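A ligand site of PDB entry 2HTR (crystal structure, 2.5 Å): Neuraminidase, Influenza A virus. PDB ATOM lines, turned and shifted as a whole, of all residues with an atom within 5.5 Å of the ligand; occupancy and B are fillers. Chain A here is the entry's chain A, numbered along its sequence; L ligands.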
ATOM      1  N   ARG A  36     -20.853   8.884  -7.549  1.00  0.00           N
ATOM      2  CA  ARG A  36     -21.766   9.059  -8.652  1.00  0.00           C
ATOM      3  C   ARG A  36     -21.339  10.413  -9.225  1.00  0.00           C
ATOM      4  O   ARG A  36     -20.705  11.209  -8.526  1.00  0.00           O
ATOM      5  CB  ARG A  36     -23.190   9.088  -8.092  1.00  0.00           C
ATOM      6  CG  ARG A  36     -24.306   8.952  -9.107  1.00  0.00           C
ATOM      7  CD  ARG A  36     -24.260   7.676  -9.920  1.00  0.00           C
ATOM      8  NE  ARG A  36     -24.360   8.032 -11.328  1.00  0.00           N
ATOM      9  CZ  ARG A  36     -25.436   8.583 -11.880  1.00  0.00           C
ATOM     10  NH1 ARG A  36     -25.419   8.907 -13.166  1.00  0.00           N
ATOM     11  NH2 ARG A  36     -26.540   8.784 -11.169  1.00  0.00           N
ATOM     12  N   GLU A  37     -21.672  10.663 -10.494  1.00  0.00           N
ATOM     13  CA  GLU A  37     -21.304  11.919 -11.157  1.00  0.00           C
ATOM     14  C   GLU A  37     -19.800  12.239 -11.143  1.00  0.00           C
ATOM     15  O   GLU A  37     -19.417  13.345 -10.765  1.00  0.00           O
ATOM     16  CB  GLU A  37     -22.050  13.124 -10.537  1.00  0.00           C
ATOM     17  CG  GLU A  37     -23.556  13.113 -10.675  1.00  0.00           C
ATOM     18  CD  GLU A  37     -24.223  12.104  -9.768  1.00  0.00           C
ATOM     19  OE1 GLU A  37     -23.791  11.974  -8.603  1.00  0.00           O
ATOM     20  OE2 GLU A  37     -25.192  11.449 -10.200  1.00  0.00           O
ATOM     21  N   LYS A  68     -30.770   7.948  -4.142  1.00  0.00           N
ATOM     22  CA  LYS A  68     -31.593   9.163  -4.084  1.00  0.00           C
ATOM     23  C   LYS A  68     -31.113  10.428  -4.791  1.00  0.00           C
ATOM     24  O   LYS A  68     -31.929  11.308  -5.090  1.00  0.00           O
ATOM     25  CB  LYS A  68     -31.909   9.507  -2.616  1.00  0.00           C
ATOM     26  CG  LYS A  68     -30.702   9.581  -1.699  1.00  0.00           C
ATOM     27  CD  LYS A  68     -31.154   9.918  -0.287  1.00  0.00           C
ATOM     28  CE  LYS A  68     -30.003   9.802   0.695  1.00  0.00           C
ATOM     29  NZ  LYS A  68     -30.407  10.104   2.100  1.00  0.00           N
ATOM     30  N   ASP A  69     -29.813  10.519  -5.066  1.00  0.00           N
ATOM     31  CA  ASP A  69     -29.228  11.668  -5.757  1.00  0.00           C
ATOM     32  C   ASP A  69     -28.881  12.876  -4.892  1.00  0.00           C
ATOM     33  O   ASP A  69     -27.987  13.639  -5.253  1.00  0.00           O
ATOM     34  CB  ASP A  69     -30.142  12.137  -6.887  1.00  0.00           C
ATOM     35  CG  ASP A  69     -30.213  11.153  -8.033  1.00  0.00           C
ATOM     36  OD1 ASP A  69     -29.155  10.583  -8.371  1.00  0.00           O
ATOM     37  OD2 ASP A  69     -31.312  10.958  -8.586  1.00  0.00           O
ATOM     38  N   ARG A  70     -29.583  13.061  -3.782  1.00  0.00           N
ATOM     39  CA  ARG A  70     -29.308  14.204  -2.916  1.00  0.00           C
ATOM     40  C   ARG A  70     -29.460  13.836  -1.456  1.00  0.00           C
ATOM     41  O   ARG A  70     -30.199  12.912  -1.106  1.00  0.00           O
ATOM     42  CB  ARG A  70     -30.251  15.377  -3.239  1.00  0.00           C
ATOM     43  CG  ARG A  70     -30.145  15.864  -4.668  1.00  0.00           C
ATOM     44  CD  ARG A  70     -31.013  17.095  -4.939  1.00  0.00           C
ATOM     45  NE  ARG A  70     -32.433  16.838  -4.745  1.00  0.00           N
ATOM     46  CZ  ARG A  70     -33.182  16.048  -5.498  1.00  0.00           C
ATOM     47  NH1 ARG A  70     -34.468  15.888  -5.213  1.00  0.00           N
ATOM     48  NH2 ARG A  70     -32.663  15.408  -6.529  1.00  0.00           N
ATOM     49  N   ARG A  74     -23.961  14.323   1.038  1.00  0.00           N
ATOM     50  CA  ARG A  74     -23.390  14.426  -0.305  1.00  0.00           C
ATOM     51  C   ARG A  74     -22.254  15.457  -0.312  1.00  0.00           C
ATOM     52  O   ARG A  74     -22.448  16.613   0.037  1.00  0.00           O
ATOM     53  CB  ARG A  74     -24.497  14.843  -1.287  1.00  0.00           C
ATOM     54  CG  ARG A  74     -24.418  14.206  -2.650  1.00  0.00           C
ATOM     55  CD  ARG A  74     -24.805  12.746  -2.607  1.00  0.00           C
ATOM     56  NE  ARG A  74     -24.214  12.019  -3.735  1.00  0.00           N
ATOM     57  CZ  ARG A  74     -24.526  12.214  -5.010  1.00  0.00           C
ATOM     58  NH1 ARG A  74     -23.925  11.501  -5.953  1.00  0.00           N
ATOM     59  NH2 ARG A  74     -25.457  13.112  -5.334  1.00  0.00           N
ATOM     60  N   TRP A  97     -24.392  18.147  -3.761  1.00  0.00           N
ATOM     61  CA  TRP A  97     -25.074  16.982  -4.287  1.00  0.00           C
ATOM     62  C   TRP A  97     -25.240  17.245  -5.785  1.00  0.00           C
ATOM     63  O   TRP A  97     -26.020  16.591  -6.472  1.00  0.00           O
ATOM     64  CB  TRP A  97     -26.436  16.698  -3.607  1.00  0.00           C
ATOM     65  CG  TRP A  97     -27.282  17.868  -3.184  1.00  0.00           C
ATOM     66  CD1 TRP A  97     -27.624  18.209  -1.899  1.00  0.00           C
ATOM     67  CD2 TRP A  97     -27.982  18.786  -4.032  1.00  0.00           C
ATOM     68  NE1 TRP A  97     -28.493  19.270  -1.893  1.00  0.00           N
ATOM     69  CE2 TRP A  97     -28.735  19.650  -3.192  1.00  0.00           C
ATOM     70  CE3 TRP A  97     -28.049  18.976  -5.415  1.00  0.00           C
ATOM     71  CZ2 TRP A  97     -29.551  20.668  -3.689  1.00  0.00           C
ATOM     72  CZ3 TRP A  97     -28.865  19.995  -5.912  1.00  0.00           C
ATOM     73  CH2 TRP A  97     -29.600  20.829  -5.051  1.00  0.00           C
ATOM     74  N   SER A  98     -24.477  18.223  -6.248  1.00  0.00           N
ATOM     75  CA  SER A  98     -24.393  18.659  -7.650  1.00  0.00           C
ATOM     76  C   SER A  98     -23.205  19.633  -7.712  1.00  0.00           C
ATOM     77  O   SER A  98     -23.165  20.591  -6.944  1.00  0.00           O
ATOM     78  CB  SER A  98     -25.676  19.368  -8.092  1.00  0.00           C
ATOM     79  OG  SER A  98     -25.547  19.853  -9.421  1.00  0.00           O
ATOM     80  N   ILE A 141     -34.692  22.774  -6.955  1.00  0.00           N
ATOM     81  CA  ILE A 141     -33.473  22.016  -7.205  1.00  0.00           C
ATOM     82  C   ILE A 141     -32.448  22.743  -8.082  1.00  0.00           C
ATOM     83  O   ILE A 141     -32.270  22.395  -9.246  1.00  0.00           O
ATOM     84  CB  ILE A 141     -33.786  20.624  -7.831  1.00  0.00           C
ATOM     85  CG1 ILE A 141     -34.795  19.869  -6.963  1.00  0.00           C
ATOM     86  CG2 ILE A 141     -32.519  19.782  -7.918  1.00  0.00           C
ATOM     87  CD1 ILE A 141     -35.118  18.473  -7.458  1.00  0.00           C
ATOM     88  N   LEU A 142     -31.776  23.736  -7.528  1.00  0.00           N
ATOM     89  CA  LEU A 142     -30.747  24.462  -8.269  1.00  0.00           C
ATOM     90  C   LEU A 142     -29.685  23.416  -8.586  1.00  0.00           C
ATOM     91  O   LEU A 142     -29.269  22.682  -7.697  1.00  0.00           O
ATOM     92  CB  LEU A 142     -30.138  25.569  -7.403  1.00  0.00           C
ATOM     93  CG  LEU A 142     -28.852  26.255  -7.869  1.00  0.00           C
ATOM     94  CD1 LEU A 142     -29.119  27.056  -9.141  1.00  0.00           C
ATOM     95  CD2 LEU A 142     -28.340  27.167  -6.758  1.00  0.00           C
ATOM     96  N   ARG A 143     -29.260  23.336  -9.841  1.00  0.00           N
ATOM     97  CA  ARG A 143     -28.268  22.344 -10.234  1.00  0.00           C
ATOM     98  C   ARG A 143     -27.271  22.855 -11.260  1.00  0.00           C
ATOM     99  O   ARG A 143     -27.472  23.915 -11.852  1.00  0.00           O
ATOM    100  CB  ARG A 143     -28.974  21.094 -10.758  1.00  0.00           C
ATOM    101  CG  ARG A 143     -30.166  21.366 -11.675  1.00  0.00           C
ATOM    102  CD  ARG A 143     -31.085  20.154 -11.756  1.00  0.00           C
ATOM    103  NE  ARG A 143     -32.105  20.258 -12.804  1.00  0.00           N
ATOM    104  CZ  ARG A 143     -33.182  21.039 -12.736  1.00  0.00           C
ATOM    105  NH1 ARG A 143     -34.044  21.047 -13.756  1.00  0.00           N
ATOM    106  NH2 ARG A 143     -33.409  21.799 -11.674  1.00  0.00           N
ATOM    107  N   GLU A 146     -22.000  18.958 -13.358  1.00  0.00           N
ATOM    108  CA  GLU A 146     -21.589  17.609 -12.978  1.00  0.00           C
ATOM    109  C   GLU A 146     -20.452  17.276 -13.937  1.00  0.00           C
ATOM    110  O   GLU A 146     -20.175  16.122 -14.235  1.00  0.00           O
ATOM    111  CB  GLU A 146     -22.727  16.589 -13.142  1.00  0.00           C
ATOM    112  CG  GLU A 146     -24.051  17.038 -12.536  1.00  0.00           C
ATOM    113  CD  GLU A 146     -23.950  17.406 -11.063  1.00  0.00           C
ATOM    114  OE1 GLU A 146     -22.843  17.694 -10.584  1.00  0.00           O
ATOM    115  OE2 GLU A 146     -24.992  17.425 -10.385  1.00  0.00           O
ATOM    116  N   ALA A 165     -37.890  19.083 -13.757  1.00  0.00           N
ATOM    117  CA  ALA A 165     -37.129  18.162 -14.598  1.00  0.00           C
ATOM    118  C   ALA A 165     -37.909  17.795 -15.850  1.00  0.00           C
ATOM    119  O   ALA A 165     -37.381  17.166 -16.769  1.00  0.00           O
ATOM    120  CB  ALA A 165     -36.781  16.911 -13.818  1.00  0.00           C
ATOM    121  N   HIS A 193     -35.116  22.454 -23.091  1.00  0.00           N
ATOM    122  CA  HIS A 193     -34.684  22.150 -21.722  1.00  0.00           C
ATOM    123  C   HIS A 193     -33.155  21.974 -21.700  1.00  0.00           C
ATOM    124  O   HIS A 193     -32.589  21.416 -22.633  1.00  0.00           O
ATOM    125  CB  HIS A 193     -35.402  20.877 -21.254  1.00  0.00           C
ATOM    126  CG  HIS A 193     -35.337  20.633 -19.785  1.00  0.00           C
ATOM    127  ND1 HIS A 193     -34.633  19.586 -19.230  1.00  0.00           N
ATOM    128  CD2 HIS A 193     -35.927  21.275 -18.745  1.00  0.00           C
ATOM    129  CE1 HIS A 193     -34.790  19.595 -17.919  1.00  0.00           C
ATOM    130  NE2 HIS A 193     -35.577  20.610 -17.598  1.00  0.00           N
ATOM    131  N   GLU A 195     -29.658  20.917 -19.151  1.00  0.00           N
ATOM    132  CA  GLU A 195     -29.147  20.339 -17.928  1.00  0.00           C
ATOM    133  C   GLU A 195     -27.801  19.663 -18.135  1.00  0.00           C
ATOM    134  O   GLU A 195     -27.486  19.219 -19.243  1.00  0.00           O
ATOM    135  CB  GLU A 195     -30.109  19.266 -17.401  1.00  0.00           C
ATOM    136  CG  GLU A 195     -31.326  19.769 -16.666  1.00  0.00           C
ATOM    137  CD  GLU A 195     -32.151  18.620 -16.099  1.00  0.00           C
ATOM    138  OE1 GLU A 195     -33.069  18.888 -15.284  1.00  0.00           O
ATOM    139  OE2 GLU A 195     -31.896  17.466 -16.465  1.00  0.00           O
ATOM    140  N   GLU A 196     -27.035  19.580 -17.052  1.00  0.00           N
ATOM    141  CA  GLU A 196     -25.747  18.902 -17.041  1.00  0.00           C
ATOM    142  C   GLU A 196     -24.896  19.118 -18.295  1.00  0.00           C
ATOM    143  O   GLU A 196     -24.523  18.165 -18.978  1.00  0.00           O
ATOM    144  CB  GLU A 196     -25.988  17.408 -16.831  1.00  0.00           C
ATOM    145  CG  GLU A 196     -26.908  17.126 -15.639  1.00  0.00           C
ATOM    146  CD  GLU A 196     -27.181  15.651 -15.403  1.00  0.00           C
ATOM    147  OE1 GLU A 196     -27.609  14.957 -16.328  1.00  0.00           O
ATOM    148  OE2 GLU A 196     -26.975  15.182 -14.265  1.00  0.00           O
ATOM    149  N   ARG A 211     -28.145  18.403 -21.824  1.00  0.00           N
ATOM    150  CA  ARG A 211     -29.196  17.408 -21.743  1.00  0.00           C
ATOM    151  C   ARG A 211     -30.599  17.984 -21.595  1.00  0.00           C
ATOM    152  O   ARG A 211     -30.879  18.729 -20.663  1.00  0.00           O
ATOM    153  CB  ARG A 211     -28.912  16.458 -20.562  1.00  0.00           C
ATOM    154  CG  ARG A 211     -30.137  15.730 -19.968  1.00  0.00           C
ATOM    155  CD  ARG A 211     -29.744  14.982 -18.699  1.00  0.00           C
ATOM    156  NE  ARG A 211     -30.878  14.359 -18.003  1.00  0.00           N
ATOM    157  CZ  ARG A 211     -30.765  13.571 -16.934  1.00  0.00           C
ATOM    158  NH1 ARG A 211     -31.851  13.055 -16.369  1.00  0.00           N
ATOM    159  NH2 ARG A 211     -29.563  13.284 -16.429  1.00  0.00           N
ATOM    160  N   TYR A 264     -36.886  11.777 -20.894  1.00  0.00           N
ATOM    161  CA  TYR A 264     -35.865  11.575 -19.869  1.00  0.00           C
ATOM    162  C   TYR A 264     -34.509  12.035 -20.435  1.00  0.00           C
ATOM    163  O   TYR A 264     -34.453  12.987 -21.214  1.00  0.00           O
ATOM    164  CB  TYR A 264     -35.842  10.098 -19.450  1.00  0.00           C
ATOM    165  CG  TYR A 264     -34.993   9.781 -18.237  1.00  0.00           C
ATOM    166  CD1 TYR A 264     -35.279  10.324 -16.987  1.00  0.00           C
ATOM    167  CD2 TYR A 264     -33.943   8.866 -18.334  1.00  0.00           C
ATOM    168  CE1 TYR A 264     -34.526   9.976 -15.858  1.00  0.00           C
ATOM    169  CE2 TYR A 264     -33.184   8.510 -17.215  1.00  0.00           C
ATOM    170  CZ  TYR A 264     -33.478   9.063 -15.986  1.00  0.00           C
ATOM    171  OH  TYR A 264     -32.728   8.702 -14.896  1.00  0.00           O
ATOM    172  N   GLY A 265     -33.446  11.372 -20.026  1.00  0.00           N
ATOM    173  CA  GLY A 265     -32.130  11.732 -20.529  1.00  0.00           C
ATOM    174  C   GLY A 265     -30.985  11.268 -19.665  1.00  0.00           C
ATOM    175  O   GLY A 265     -31.172  10.683 -18.596  1.00  0.00           O
ATOM    176  N   ARG A 288     -28.818   2.581 -19.846  1.00  0.00           N
ATOM    177  CA  ARG A 288     -27.523   3.228 -19.745  1.00  0.00           C
ATOM    178  C   ARG A 288     -26.470   2.119 -19.783  1.00  0.00           C
ATOM    179  O   ARG A 288     -25.845   1.787 -18.769  1.00  0.00           O
ATOM    180  CB  ARG A 288     -27.444   4.025 -18.447  1.00  0.00           C
ATOM    181  CG  ARG A 288     -28.391   5.232 -18.428  1.00  0.00           C
ATOM    182  CD  ARG A 288     -28.271   6.035 -17.143  1.00  0.00           C
ATOM    183  NE  ARG A 288     -29.052   7.263 -17.205  1.00  0.00           N
ATOM    184  CZ  ARG A 288     -29.124   8.165 -16.225  1.00  0.00           C
ATOM    185  NH1 ARG A 288     -29.856   9.253 -16.368  1.00  0.00           N
ATOM    186  NH2 ARG A 288     -28.460   7.968 -15.091  1.00  0.00           N
ATOM    187  N   TYR A 322     -23.244   8.361 -17.353  1.00  0.00           N
ATOM    188  CA  TYR A 322     -22.789   9.715 -17.616  1.00  0.00           C
ATOM    189  C   TYR A 322     -21.485   9.783 -18.395  1.00  0.00           C
ATOM    190  O   TYR A 322     -20.718   8.828 -18.437  1.00  0.00           O
ATOM    191  CB  TYR A 322     -22.632  10.494 -16.294  1.00  0.00           C
ATOM    192  CG  TYR A 322     -23.918  11.115 -15.797  1.00  0.00           C
ATOM    193  CD1 TYR A 322     -25.159  10.614 -16.207  1.00  0.00           C
ATOM    194  CD2 TYR A 322     -23.911  12.198 -14.929  1.00  0.00           C
ATOM    195  CE1 TYR A 322     -26.340  11.168 -15.767  1.00  0.00           C
ATOM    196  CE2 TYR A 322     -25.098  12.775 -14.471  1.00  0.00           C
ATOM    197  CZ  TYR A 322     -26.311  12.247 -14.904  1.00  0.00           C
ATOM    198  OH  TYR A 322     -27.500  12.795 -14.493  1.00  0.00           O
HETATM  199  C1  LIG L   1     -29.695  10.846 -13.086  1.00  0.00           C
HETATM  200  C2  LIG L   1     -29.639  12.000 -12.245  1.00  0.00           C
HETATM  201  C3  LIG L   1     -28.609  12.068 -11.129  1.00  0.00           C
HETATM  202  C4  LIG L   1     -28.387  13.535 -10.662  1.00  0.00           C
HETATM  203  C5  LIG L   1     -29.677  14.348 -10.689  1.00  0.00           C
HETATM  204  C6  LIG L   1     -30.228  14.312 -12.126  1.00  0.00           C
HETATM  205  C7  LIG L   1     -31.533  15.079 -12.298  1.00  0.00           C
HETATM  206  C8  LIG L   1     -32.041  15.035 -13.744  1.00  0.00           C
HETATM  207  C9  LIG L   1     -33.371  15.804 -13.920  1.00  0.00           C
HETATM  208  C10 LIG L   1     -29.714  16.185  -9.041  1.00  0.00           C
HETATM  209  C11 LIG L   1     -29.312  17.592  -8.676  1.00  0.00           C
HETATM  210  N1  LIG L   1     -29.348  15.689 -10.227  1.00  0.00           N
HETATM  211  O1  LIG L   1     -28.921   9.734 -12.866  1.00  0.00           O
HETATM  212  O2  LIG L   1     -30.512  10.828 -14.092  1.00  0.00           O
HETATM  213  O3  LIG L   1     -27.838  13.503  -9.339  1.00  0.00           O
HETATM  214  O4  LIG L   1     -30.485  12.937 -12.516  1.00  0.00           O
HETATM  215  O5  LIG L   1     -32.558  14.485 -11.501  1.00  0.00           O
HETATM  216  O6  LIG L   1     -31.064  15.625 -14.601  1.00  0.00           O
HETATM  217  O7  LIG L   1     -33.335  17.141 -13.492  1.00  0.00           O
HETATM  218  O8  LIG L   1     -30.437  15.472  -8.124  1.00  0.00           O
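OE1 of Glu 195 is in salt-bridge range of NH1 of Arg 143 (2.8 Å). The backbone carbonyl oxygen (O) of Gly 265 lies within hydrogen-bond range of the guanidinium group (NH1) of Arg 288, at 3.0 Å. OE2 of Glu 37 lies within salt-bridge range of NH2 of Arg 36 (3.1 Å). OH of Tyr 322 is in hydrogen-bond range of NH2 of Arg 211, 2.9 Å away. The side-chain carboxylate (OE1) of Glu 196 lies within salt-bridge range of the guanidinium group (NH2) of Arg 211 (2.6 Å). The backbone carbonyl oxygen of Gly 265 lies within hydrogen-bond range of the guanidinium group of Arg 211 (3.3 Å). O of Ile 141 sits at hydrogen-bond distance from NH2 of Arg 143 (2.7 Å). The side-chain carboxylate (OE1) of Glu 37 lies within salt-bridge range of the guanidinium group (NH1) of Arg 74 (2.7 Å).
Merely in contact with the ligand: Trp 97 (3.7 Å), Ile 141 (3.96 Å), Ala 165 (3.5 Å), Glu 196 (3.9 Å) and Tyr 322 (3.2 Å). Hydrophobic or aromatic side chains within 4 Å of the ligand: Trp 97, Ile 141, Ala 165 and Tyr 264. Of the 21 residues printed, 14 come within 4 Å of the ligand.
An oxygen (O7) of the ligand lies within hydrogen-bond range of the side-chain carboxylate (OE1) of Glu 195, 2.5 Å away. The guanidinium group (NH2) of Arg 70 sits at hydrogen-bond distance from an oxygen (O8) of the ligand. An oxygen (O2) of the ligand is in salt-bridge range of the guanidinium group (NH1) of Arg 288. The guanidinium group (NH2) of Arg 36 lies within salt-bridge range of an oxygen (O1) of the ligand, 3.1 Å away. The guanidinium group (NH1) of Arg 211 lies within salt-bridge range of an oxygen (O2) of the ligand, at 3.5 Å. The side-chain hydroxyl (OH) of Tyr 264 sits at hydrogen-bond distance from an oxygen (O2) of the ligand (3.2 Å). The side-chain carboxylate (OD1) of Asp 69 sits close to an oxygen (O3) of the ligand (3.3 Å). NE of Arg 143 lies within hydrogen-bond range of O7 of the ligand (3.4 Å). The side-chain carboxylate (OE2) of Glu 37 is in hydrogen-bond range of an oxygen (O3) of the ligand, at 3.5 Å.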
